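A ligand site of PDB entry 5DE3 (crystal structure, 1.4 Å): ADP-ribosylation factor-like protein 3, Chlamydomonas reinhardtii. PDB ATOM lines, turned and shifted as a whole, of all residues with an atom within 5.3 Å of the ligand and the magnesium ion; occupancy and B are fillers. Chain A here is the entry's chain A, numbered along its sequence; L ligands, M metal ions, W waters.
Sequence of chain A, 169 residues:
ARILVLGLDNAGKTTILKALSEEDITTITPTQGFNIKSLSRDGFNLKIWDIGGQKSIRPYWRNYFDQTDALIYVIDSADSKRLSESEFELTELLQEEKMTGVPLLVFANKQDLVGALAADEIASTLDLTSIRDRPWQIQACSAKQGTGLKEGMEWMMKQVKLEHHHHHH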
ATOM      1  N   GLY A   7      27.095  15.225  -8.095  1.00  0.00           N
ATOM      2  CA  GLY A   7      27.483  15.781  -9.384  1.00  0.00           C
ATOM      3  C   GLY A   7      26.390  16.675  -9.957  1.00  0.00           C
ATOM      4  O   GLY A   7      25.228  16.592  -9.513  1.00  0.00           O
ATOM      5  N   LEU A   8      26.728  17.541 -10.922  1.00  0.00           N
ATOM      6  CA  LEU A   8      25.733  18.451 -11.512  1.00  0.00           C
ATOM      7  C   LEU A   8      24.582  17.709 -12.203  1.00  0.00           C
ATOM      8  O   LEU A   8      24.702  16.539 -12.596  1.00  0.00           O
ATOM      9  CB  LEU A   8      26.394  19.396 -12.534  1.00  0.00           C
ATOM     10  CG  LEU A   8      27.611  20.221 -12.095  1.00  0.00           C
ATOM     11  CD1 LEU A   8      28.045  21.104 -13.270  1.00  0.00           C
ATOM     12  CD2 LEU A   8      27.367  21.061 -10.855  1.00  0.00           C
ATOM     13  N   ASP A   9      23.447  18.404 -12.342  1.00  0.00           N
ATOM     14  CA  ASP A   9      22.361  17.921 -13.194  1.00  0.00           C
ATOM     15  C   ASP A   9      22.900  17.574 -14.594  1.00  0.00           C
ATOM     16  O   ASP A   9      23.808  18.256 -15.093  1.00  0.00           O
ATOM     17  CB  ASP A   9      21.246  18.962 -13.267  1.00  0.00           C
ATOM     18  CG  ASP A   9      21.762  20.354 -13.671  1.00  0.00           C
ATOM     19  OD1 ASP A   9      22.458  21.012 -12.847  1.00  0.00           O
ATOM     20  OD2 ASP A   9      21.491  20.789 -14.812  1.00  0.00           O
ATOM     21  N   ASN A  10      22.372  16.496 -15.186  1.00  0.00           N
ATOM     22  CA  ASN A  10      22.714  16.008 -16.525  1.00  0.00           C
ATOM     23  C   ASN A  10      24.072  15.272 -16.640  1.00  0.00           C
ATOM     24  O   ASN A  10      24.463  14.884 -17.747  1.00  0.00           O
ATOM     25  CB  ASN A  10      22.660  17.144 -17.565  1.00  0.00           C
ATOM     26  CG  ASN A  10      22.441  16.649 -18.999  1.00  0.00           C
ATOM     27  OD1 ASN A  10      21.549  15.832 -19.256  1.00  0.00           O
ATOM     28  ND2 ASN A  10      23.255  17.144 -19.927  1.00  0.00           N
ATOM     29  N   ALA A  11      24.773  15.058 -15.523  1.00  0.00           N
ATOM     30  CA  ALA A  11      26.096  14.417 -15.569  1.00  0.00           C
ATOM     31  C   ALA A  11      26.030  12.933 -15.893  1.00  0.00           C
ATOM     32  O   ALA A  11      26.967  12.370 -16.482  1.00  0.00           O
ATOM     33  CB  ALA A  11      26.838  14.610 -14.242  1.00  0.00           C
ATOM     34  N   GLY A  12      24.917  12.310 -15.491  1.00  0.00           N
ATOM     35  CA  GLY A  12      24.656  10.901 -15.758  1.00  0.00           C
ATOM     36  C   GLY A  12      24.600   9.978 -14.554  1.00  0.00           C
ATOM     37  O   GLY A  12      24.818   8.761 -14.685  1.00  0.00           O
ATOM     38  N   LYS A  13      24.298  10.542 -13.387  1.00  0.00           N
ATOM     39  CA  LYS A  13      24.248   9.789 -12.128  1.00  0.00           C
ATOM     40  C   LYS A  13      23.242   8.620 -12.143  1.00  0.00           C
ATOM     41  O   LYS A  13      23.565   7.488 -11.754  1.00  0.00           O
ATOM     42  CB  LYS A  13      23.943  10.733 -10.958  1.00  0.00           C
ATOM     43  CG  LYS A  13      25.028  11.821 -10.733  1.00  0.00           C
ATOM     44  CD  LYS A  13      24.718  12.786  -9.571  1.00  0.00           C
ATOM     45  CE  LYS A  13      23.415  13.586  -9.749  1.00  0.00           C
ATOM     46  NZ  LYS A  13      23.436  14.521 -10.907  1.00  0.00           N
ATOM     47  N   THR A  14      22.010   8.896 -12.585  1.00  0.00           N
ATOM     48  CA  THR A  14      20.969   7.882 -12.555  1.00  0.00           C
ATOM     49  C   THR A  14      21.214   6.814 -13.627  1.00  0.00           C
ATOM     50  O   THR A  14      20.956   5.616 -13.400  1.00  0.00           O
ATOM     51  CB  THR A  14      19.590   8.525 -12.738  1.00  0.00           C
ATOM     52  OG1 THR A  14      19.377   9.508 -11.722  1.00  0.00           O
ATOM     53  CG2 THR A  14      18.474   7.463 -12.677  1.00  0.00           C
ATOM     54  N   THR A  15      21.726   7.234 -14.779  1.00  0.00           N
ATOM     55  CA  THR A  15      22.076   6.294 -15.839  1.00  0.00           C
ATOM     56  C   THR A  15      23.167   5.316 -15.369  1.00  0.00           C
ATOM     57  O   THR A  15      23.086   4.109 -15.656  1.00  0.00           O
ATOM     58  CB  THR A  15      22.524   7.056 -17.123  1.00  0.00           C
ATOM     59  OG1 THR A  15      21.476   7.942 -17.529  1.00  0.00           O
ATOM     60  CG2 THR A  15      22.824   6.084 -18.269  1.00  0.00           C
ATOM     61  N   ILE A  16      24.168   5.804 -14.622  1.00  0.00           N
ATOM     62  CA  ILE A  16      25.216   4.929 -14.096  1.00  0.00           C
ATOM     63  C   ILE A  16      24.605   3.909 -13.140  1.00  0.00           C
ATOM     64  O   ILE A  16      24.910   2.712 -13.215  1.00  0.00           O
ATOM     65  CB  ILE A  16      26.354   5.746 -13.394  1.00  0.00           C
ATOM     66  CG1 ILE A  16      27.220   6.444 -14.465  1.00  0.00           C
ATOM     67  CG2 ILE A  16      27.184   4.843 -12.461  1.00  0.00           C
ATOM     68  CD1 ILE A  16      28.281   7.427 -13.906  1.00  0.00           C
ATOM     69  N   ILE A  25      17.821   2.155 -19.460  1.00  0.00           N
ATOM     70  CA  ILE A  25      18.098   3.576 -19.330  1.00  0.00           C
ATOM     71  C   ILE A  25      17.275   4.448 -20.298  1.00  0.00           C
ATOM     72  O   ILE A  25      17.327   5.663 -20.193  1.00  0.00           O
ATOM     73  CB  ILE A  25      19.587   3.893 -19.554  1.00  0.00           C
ATOM     74  CG1 ILE A  25      19.991   3.638 -21.003  1.00  0.00           C
ATOM     75  CG2 ILE A  25      20.447   3.081 -18.586  1.00  0.00           C
ATOM     76  CD1 ILE A  25      21.462   3.897 -21.264  1.00  0.00           C
ATOM     77  N   ILE A  28      14.722   7.117 -18.393  1.00  0.00           N
ATOM     78  CA  ILE A  28      15.198   7.939 -17.271  1.00  0.00           C
ATOM     79  C   ILE A  28      14.816   9.411 -17.443  1.00  0.00           C
ATOM     80  O   ILE A  28      14.976   9.995 -18.512  1.00  0.00           O
ATOM     81  CB  ILE A  28      16.735   7.817 -17.107  1.00  0.00           C
ATOM     82  CG1 ILE A  28      17.106   6.371 -16.750  1.00  0.00           C
ATOM     83  CG2 ILE A  28      17.244   8.757 -16.037  1.00  0.00           C
ATOM     84  CD1 ILE A  28      18.600   6.139 -16.691  1.00  0.00           C
ATOM     85  N   THR A  29      14.296  10.002 -16.370  1.00  0.00           N
ATOM     86  CA  THR A  29      13.947  11.410 -16.358  1.00  0.00           C
ATOM     87  C   THR A  29      14.742  12.117 -15.239  1.00  0.00           C
ATOM     88  O   THR A  29      15.247  11.444 -14.344  1.00  0.00           O
ATOM     89  CB  THR A  29      12.419  11.604 -16.149  1.00  0.00           C
ATOM     90  OG1 THR A  29      12.042  11.151 -14.845  1.00  0.00           O
ATOM     91  CG2 THR A  29      11.633  10.830 -17.200  1.00  0.00           C
ATOM     92  N   PRO A  30      14.869  13.455 -15.312  1.00  0.00           N
ATOM     93  CA  PRO A  30      15.573  14.175 -14.249  1.00  0.00           C
ATOM     94  C   PRO A  30      15.053  13.830 -12.852  1.00  0.00           C
ATOM     95  O   PRO A  30      13.848  13.698 -12.651  1.00  0.00           O
ATOM     96  CB  PRO A  30      15.292  15.644 -14.574  1.00  0.00           C
ATOM     97  CG  PRO A  30      15.126  15.661 -16.038  1.00  0.00           C
ATOM     98  CD  PRO A  30      14.444  14.373 -16.391  1.00  0.00           C
ATOM     99  N   THR A  31      15.966  13.685 -11.908  1.00  0.00           N
ATOM    100  CA  THR A  31      15.617  13.250 -10.565  1.00  0.00           C
ATOM    101  C   THR A  31      15.179  14.409  -9.671  1.00  0.00           C
ATOM    102  O   THR A  31      15.983  15.299  -9.338  1.00  0.00           O
ATOM    103  CB  THR A  31      16.804  12.511  -9.924  1.00  0.00           C
ATOM    104  OG1 THR A  31      17.214  11.452 -10.793  1.00  0.00           O
ATOM    105  CG2 THR A  31      16.438  11.921  -8.572  1.00  0.00           C
ATOM    106  N   ASN A  35      17.201   8.798  -5.458  1.00  0.00           N
ATOM    107  CA  ASN A  35      16.953   7.372  -5.647  1.00  0.00           C
ATOM    108  C   ASN A  35      17.799   6.527  -4.691  1.00  0.00           C
ATOM    109  O   ASN A  35      18.925   6.899  -4.363  1.00  0.00           O
ATOM    110  CB  ASN A  35      17.252   6.953  -7.099  1.00  0.00           C
ATOM    111  CG  ASN A  35      16.414   7.697  -8.108  1.00  0.00           C
ATOM    112  OD1 ASN A  35      15.194   7.842  -7.934  1.00  0.00           O
ATOM    113  ND2 ASN A  35      17.040   8.166  -9.174  1.00  0.00           N
ATOM    114  N   ASP A  50      21.505   8.134  -4.845  1.00  0.00           N
ATOM    115  CA  ASP A  50      21.693   8.989  -6.030  1.00  0.00           C
ATOM    116  C   ASP A  50      20.839  10.269  -5.898  1.00  0.00           C
ATOM    117  O   ASP A  50      19.611  10.198  -6.032  1.00  0.00           O
ATOM    118  CB  ASP A  50      21.333   8.173  -7.291  1.00  0.00           C
ATOM    119  CG  ASP A  50      20.889   9.020  -8.479  1.00  0.00           C
ATOM    120  OD1 ASP A  50      21.401  10.133  -8.677  1.00  0.00           O
ATOM    121  OD2 ASP A  50      20.007   8.526  -9.251  1.00  0.00           O
ATOM    122  N   ILE A  51      21.464  11.413  -5.596  1.00  0.00           N
ATOM    123  CA  ILE A  51      20.725  12.646  -5.281  1.00  0.00           C
ATOM    124  C   ILE A  51      20.610  13.554  -6.503  1.00  0.00           C
ATOM    125  O   ILE A  51      21.581  13.730  -7.239  1.00  0.00           O
ATOM    126  CB  ILE A  51      21.393  13.462  -4.135  1.00  0.00           C
ATOM    127  CG1 ILE A  51      22.012  12.562  -3.047  1.00  0.00           C
ATOM    128  CG2 ILE A  51      20.399  14.465  -3.527  1.00  0.00           C
ATOM    129  CD1 ILE A  51      21.003  11.667  -2.299  1.00  0.00           C
ATOM    130  N   GLY A  52      19.428  14.135  -6.724  1.00  0.00           N
ATOM    131  CA  GLY A  52      19.240  15.029  -7.861  1.00  0.00           C
ATOM    132  C   GLY A  52      20.185  16.230  -7.820  1.00  0.00           C
ATOM    133  O   GLY A  52      20.470  16.737  -6.735  1.00  0.00           O
ATOM    134  N   GLY A  53      20.668  16.679  -8.978  1.00  0.00           N
ATOM    135  CA  GLY A  53      21.695  17.709  -9.036  1.00  0.00           C
ATOM    136  C   GLY A  53      21.307  19.109  -9.489  1.00  0.00           C
ATOM    137  O   GLY A  53      22.166  19.980  -9.552  1.00  0.00           O
ATOM    138  N   GLN A  54      20.026  19.340  -9.818  1.00  0.00           N
ATOM    139  CA  GLN A  54      19.591  20.697 -10.193  1.00  0.00           C
ATOM    140  C   GLN A  54      19.877  21.669  -9.053  1.00  0.00           C
ATOM    141  O   GLN A  54      19.729  21.307  -7.889  1.00  0.00           O
ATOM    142  CB  GLN A  54      18.091  20.701 -10.539  1.00  0.00           C
ATOM    143  CG  GLN A  54      17.795  20.156 -11.905  1.00  0.00           C
ATOM    144  CD  GLN A  54      18.032  21.172 -13.011  1.00  0.00           C
ATOM    145  OE1 GLN A  54      18.467  22.300 -12.754  1.00  0.00           O
ATOM    146  NE2 GLN A  54      17.750  20.777 -14.237  1.00  0.00           N
ATOM    147  N   ASN A 109      32.426  10.805 -17.143  1.00  0.00           N
ATOM    148  CA  ASN A 109      31.391  10.080 -17.903  1.00  0.00           C
ATOM    149  C   ASN A 109      31.194  10.590 -19.347  1.00  0.00           C
ATOM    150  O   ASN A 109      31.690  11.670 -19.712  1.00  0.00           O
ATOM    151  CB  ASN A 109      30.063  10.135 -17.123  1.00  0.00           C
ATOM    152  CG  ASN A 109      28.986   9.153 -17.667  1.00  0.00           C
ATOM    153  OD1 ASN A 109      29.287   8.042 -18.131  1.00  0.00           O
ATOM    154  ND2 ASN A 109      27.734   9.577 -17.582  1.00  0.00           N
ATOM    155  N   LYS A 110      30.477   9.798 -20.155  1.00  0.00           N
ATOM    156  CA  LYS A 110      30.116  10.154 -21.547  1.00  0.00           C
ATOM    157  C   LYS A 110      31.316  10.196 -22.497  1.00  0.00           C
ATOM    158  O   LYS A 110      31.386  11.042 -23.392  1.00  0.00           O
ATOM    159  CB  LYS A 110      29.372  11.496 -21.621  1.00  0.00           C
ATOM    160  CG  LYS A 110      28.167  11.593 -20.663  1.00  0.00           C
ATOM    161  CD  LYS A 110      27.216  12.722 -21.062  1.00  0.00           C
ATOM    162  CE  LYS A 110      26.116  12.958 -20.021  1.00  0.00           C
ATOM    163  NZ  LYS A 110      25.219  14.121 -20.420  1.00  0.00           N
ATOM    164  N   GLN A 111      32.254   9.266 -22.313  1.00  0.00           N
ATOM    165  CA  GLN A 111      33.447   9.171 -23.163  1.00  0.00           C
ATOM    166  C   GLN A 111      33.092   8.779 -24.603  1.00  0.00           C
ATOM    167  O   GLN A 111      33.935   8.898 -25.501  1.00  0.00           O
ATOM    168  CB  GLN A 111      34.450   8.170 -22.569  1.00  0.00           C
ATOM    169  CG  GLN A 111      35.115   8.623 -21.255  1.00  0.00           C
ATOM    170  CD  GLN A 111      36.086   9.773 -21.463  1.00  0.00           C
ATOM    171  OE1 GLN A 111      37.003   9.689 -22.288  1.00  0.00           O
ATOM    172  NE2 GLN A 111      35.898  10.858 -20.718  1.00  0.00           N
ATOM    173  N   ASP A 112      31.864   8.315 -24.809  1.00  0.00           N
ATOM    174  CA  ASP A 112      31.387   7.913 -26.130  1.00  0.00           C
ATOM    175  C   ASP A 112      31.059   9.107 -27.033  1.00  0.00           C
ATOM    176  O   ASP A 112      30.938   8.960 -28.245  1.00  0.00           O
ATOM    177  CB  ASP A 112      30.140   7.026 -26.001  1.00  0.00           C
ATOM    178  CG  ASP A 112      28.985   7.720 -25.305  1.00  0.00           C
ATOM    179  OD1 ASP A 112      28.984   7.776 -24.049  1.00  0.00           O
ATOM    180  OD2 ASP A 112      28.075   8.222 -25.997  1.00  0.00           O
ATOM    181  N   LEU A 113      30.918  10.297 -26.439  1.00  0.00           N
ATOM    182  CA  LEU A 113      30.573  11.491 -27.213  1.00  0.00           C
ATOM    183  C   LEU A 113      31.785  12.194 -27.821  1.00  0.00           C
ATOM    184  O   LEU A 113      32.890  12.203 -27.245  1.00  0.00           O
ATOM    185  CB  LEU A 113      29.789  12.485 -26.341  1.00  0.00           C
ATOM    186  CG  LEU A 113      28.387  12.066 -25.900  1.00  0.00           C
ATOM    187  CD1 LEU A 113      27.770  13.121 -25.004  1.00  0.00           C
ATOM    188  CD2 LEU A 113      27.512  11.809 -27.126  1.00  0.00           C
ATOM    189  N   CYS A 141      34.688   6.717 -18.159  1.00  0.00           N
ATOM    190  CA  CYS A 141      33.601   5.748 -18.382  1.00  0.00           C
ATOM    191  C   CYS A 141      32.533   6.211 -19.377  1.00  0.00           C
ATOM    192  O   CYS A 141      32.457   7.384 -19.748  1.00  0.00           O
ATOM    193  CB  CYS A 141      32.918   5.394 -17.047  1.00  0.00           C
ATOM    194  SG  CYS A 141      32.009   6.749 -16.238  1.00  0.00           S
ATOM    195  N   SER A 142      31.706   5.259 -19.804  1.00  0.00           N
ATOM    196  CA  SER A 142      30.505   5.524 -20.590  1.00  0.00           C
ATOM    197  C   SER A 142      29.351   4.681 -20.045  1.00  0.00           C
ATOM    198  O   SER A 142      29.353   3.454 -20.183  1.00  0.00           O
ATOM    199  CB  SER A 142      30.711   5.212 -22.081  1.00  0.00           C
ATOM    200  OG  SER A 142      29.469   5.234 -22.773  1.00  0.00           O
ATOM    201  N   ALA A 143      28.378   5.340 -19.437  1.00  0.00           N
ATOM    202  CA  ALA A 143      27.251   4.633 -18.851  1.00  0.00           C
ATOM    203  C   ALA A 143      26.353   4.013 -19.921  1.00  0.00           C
ATOM    204  O   ALA A 143      25.663   3.023 -19.684  1.00  0.00           O
ATOM    205  CB  ALA A 143      26.442   5.551 -17.966  1.00  0.00           C
ATOM    206  N   LYS A 144      26.363   4.608 -21.112  1.00  0.00           N
ATOM    207  CA  LYS A 144      25.499   4.130 -22.185  1.00  0.00           C
ATOM    208  C   LYS A 144      26.064   2.833 -22.736  1.00  0.00           C
ATOM    209  O   LYS A 144      25.326   2.037 -23.329  1.00  0.00           O
ATOM    210  CB  LYS A 144      25.383   5.166 -23.300  1.00  0.00           C
ATOM    211  CG  LYS A 144      24.819   4.648 -24.628  1.00  0.00           C
ATOM    212  CD  LYS A 144      24.522   5.803 -25.553  1.00  0.00           C
ATOM    213  CE  LYS A 144      24.083   5.319 -26.923  1.00  0.00           C
ATOM    214  NZ  LYS A 144      24.894   4.158 -27.377  1.00  0.00           N
HETATM  215  P1  LIG L   1      19.812  14.721 -12.481  1.00  0.00           P
HETATM  216  O1  LIG L   1      18.838  13.603 -12.132  1.00  0.00           O
HETATM  217  O2  LIG L   1      19.160  16.043 -12.812  1.00  0.00           O
HETATM  218  O3  LIG L   1      20.760  14.822 -11.276  1.00  0.00           O
HETATM  219  N1  LIG L   1      20.674  14.236 -13.728  1.00  0.00           N
HETATM  220  P2  LIG L   1      21.565  12.896 -13.810  1.00  0.00           P
HETATM  221  O4  LIG L   1      20.898  11.818 -13.045  1.00  0.00           O
HETATM  222  O5  LIG L   1      23.000  13.206 -13.431  1.00  0.00           O
HETATM  223  O6  LIG L   1      21.628  12.466 -15.296  1.00  0.00           O
HETATM  224  P3  LIG L   1      20.845  11.357 -16.110  1.00  0.00           P
HETATM  225  O7  LIG L   1      19.391  11.709 -16.052  1.00  0.00           O
HETATM  226  O8  LIG L   1      21.269  10.016 -15.671  1.00  0.00           O
HETATM  227  O9  LIG L   1      21.330  11.465 -17.599  1.00  0.00           O
HETATM  228  C1  LIG L   1      21.244  12.695 -18.286  1.00  0.00           C
HETATM  229  C2  LIG L   1      21.250  12.480 -19.791  1.00  0.00           C
HETATM  230  O10 LIG L   1      22.566  12.054 -20.245  1.00  0.00           O
HETATM  231  C3  LIG L   1      20.287  11.417 -20.320  1.00  0.00           C
HETATM  232  O11 LIG L   1      19.755  11.813 -21.576  1.00  0.00           O
HETATM  233  C4  LIG L   1      21.188  10.191 -20.473  1.00  0.00           C
HETATM  234  O12 LIG L   1      20.695   9.273 -21.432  1.00  0.00           O
HETATM  235  C5  LIG L   1      22.492  10.833 -20.944  1.00  0.00           C
HETATM  236  N2  LIG L   1      23.681  10.029 -20.677  1.00  0.00           N
HETATM  237  C6  LIG L   1      24.060   9.496 -19.457  1.00  0.00           C
HETATM  238  N3  LIG L   1      25.171   8.825 -19.516  1.00  0.00           N
HETATM  239  C7  LIG L   1      25.583   8.920 -20.841  1.00  0.00           C
HETATM  240  C8  LIG L   1      26.727   8.396 -21.480  1.00  0.00           C
HETATM  241  O13 LIG L   1      27.644   7.711 -21.007  1.00  0.00           O
HETATM  242  N4  LIG L   1      26.764   8.736 -22.830  1.00  0.00           N
HETATM  243  C9  LIG L   1      25.805   9.491 -23.466  1.00  0.00           C
HETATM  244  N5  LIG L   1      26.020   9.708 -24.778  1.00  0.00           N
HETATM  245  N6  LIG L   1      24.730   9.989 -22.882  1.00  0.00           N
HETATM  246  C10 LIG L   1      24.675   9.673 -21.559  1.00  0.00           C
HETATM  247 MG    MG M   1      19.155  11.624 -11.999  1.00  0.00          MG
HETATM  248  O   HOH W   1      17.730  17.195 -10.555  1.00  0.00           O
HETATM  249  O   HOH W   2      18.251  17.492 -14.746  1.00  0.00           O
HETATM  250  O   HOH W   3      20.140  12.014 -10.036  1.00  0.00           O
HETATM  251  O   HOH W   4      17.989  11.325 -13.592  1.00  0.00           O
HETATM  252  O   HOH W   5      19.826   7.253 -19.838  1.00  0.00           O
HETATM  253  O   HOH W   6      24.166  12.991 -23.107  1.00  0.00           O
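The backbone NH (N) of Lys 13 is in hydrogen-bond range of an oxygen (O5) of the ligand, 3.0 Å away. N of Thr 31 lies close to O1 of the ligand (2.9 Å). The backbone NH (N) of Lys 144 is in hydrogen-bond range of an oxygen (O13) of the ligand (3.4 Å). The side-chain amide nitrogen of Asn 109 sits at hydrogen-bond distance from a nitrogen (N3) of the ligand (3.3 Å). N of Gly 53 lies within hydrogen-bond range of O3 of the ligand (3.0 Å). An oxygen (O8) of the ligand sits at hydrogen-bond distance from the backbone NH (N) of Thr 15 (3.0 Å). An oxygen (O5) of the ligand lies within hydrogen-bond range of the backbone NH (N) of Gly 12 (3.0 Å). O5 of the ligand sits at hydrogen-bond distance from N of Ala 11 (3.3 Å). An oxygen (O3) of the ligand lies within salt-bridge range of the side-chain amino group of Lys 13. An oxygen (O13) of the ligand sits at hydrogen-bond distance from the backbone NH (N) of Ala 143 (2.9 Å). A nitrogen (N4) of the ligand sits at hydrogen-bond distance from the side-chain carboxylate (OD1) of Asp 112. OG1 of Thr 15 is in hydrogen-bond range of O8 of the ligand. An oxygen (O8) of the ligand is in hydrogen-bond range of the backbone NH (N) of Thr 14 (3.4 Å). The side-chain amino group (NZ) of Lys 110 is in hydrogen-bond range of an oxygen (O10) of the ligand.
SG of Cys 141 lies within hydrogen-bond range of OD1 of Asn 109 (3.6 Å). The side-chain hydroxyl (OG) of Ser 142 sits at hydrogen-bond distance from the side-chain carboxylate (OD1) of Asp 112, at 2.9 Å. The backbone NH (N) of Ala 143 is in hydrogen-bond range of the side-chain amide oxygen (OD1) of Asn 109 (3.1 Å). The side-chain amino group of Lys 13 lies within hydrogen-bond range of the backbone carbonyl oxygen of Gly 7, 3.1 Å away. The backbone carbonyl oxygen (O) of Ala 11 sits at hydrogen-bond distance from the side-chain amide nitrogen (ND2) of Asn 109 (3.1 Å). O of Asn 10 sits at hydrogen-bond distance from NZ of Lys 110. The backbone NH (N) of Lys 110 sits at hydrogen-bond distance from the backbone carbonyl oxygen (O) of Cys 141, at 3.1 Å. OG1 of Thr 14 lies close to OD2 of Asp 50 (2.7 Å).
A nitrogen (N1) of the ligand sits close to the backbone NH (N) of Asn 10 (3.2 Å). Residues that only touch the ligand: Leu 8 (3.8 Å), Asp 9 (3.6 Å), Ile 28 (3.7 Å), Pro 30 (3.9 Å), Gly 52 (3.7 Å), Leu 113 (3.5 Å) and Ser 142 (3.5 Å). Hydrophobic or aromatic side chains that line the ligand: Ile 28, Leu 113 and Ala 143. Within 4 Å of the ligand: Leu 8, Asp 9, Asn 10, Ala 11, Gly 12, Lys 13, Thr 14, Thr 15, Ile 28, Pro 30, Thr 31, Gly 52, Gly 53, Asn 109, Lys 110, Asp 112, Leu 113, Ser 142, Ala 143 and Lys 144. The nearest printed residue that does not touch the ligand is Ile 51 (4.3 Å).
Two residues have an atom within 4 Å of the magnesium ion: Thr 14 and Thr 31. Along chain A the residues within 4 Å of the magnesium ion span positions 14 to 31.
The magnesium ion is bound by water W4 (2.0 Å), O1 of the ligand (2.0 Å), O4 of the ligand (2.0 Å), OG1 of Thr 14 (2.1 Å), water W3 (2.2 Å) and OG1 of Thr 31 (2.3 Å).
Water W3 bridges OD1 of Asp 50 (2.6 Å) and O3 of the ligand (3.1 Å). Water W4 lies within hydrogen-bond range of the backbone carbonyl oxygen (O) of Thr 29 (2.8 Å) and an oxygen (O7) of the ligand (2.9 Å). Water W2 lies within hydrogen-bond range of an oxygen (O2) of the ligand (2.6 Å) and the side-chain amide nitrogen (NE2) of Gln 54 (3.4 Å). Water W5 lies within hydrogen-bond range of O12 of the ligand, OG1 of Thr 15 and O of Ile 25. Water W1 lies within hydrogen-bond range of O of Thr 31 (2.9 Å), O2 of the ligand (2.9 Å), N of Gln 54 (3.2 Å) and N of Gly 53 (3.4 Å). Water W6 lies within hydrogen-bond range of a nitrogen (N6) of the ligand (3.1 Å) and the side-chain amino group (NZ) of Lys 110 (3.1 Å).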
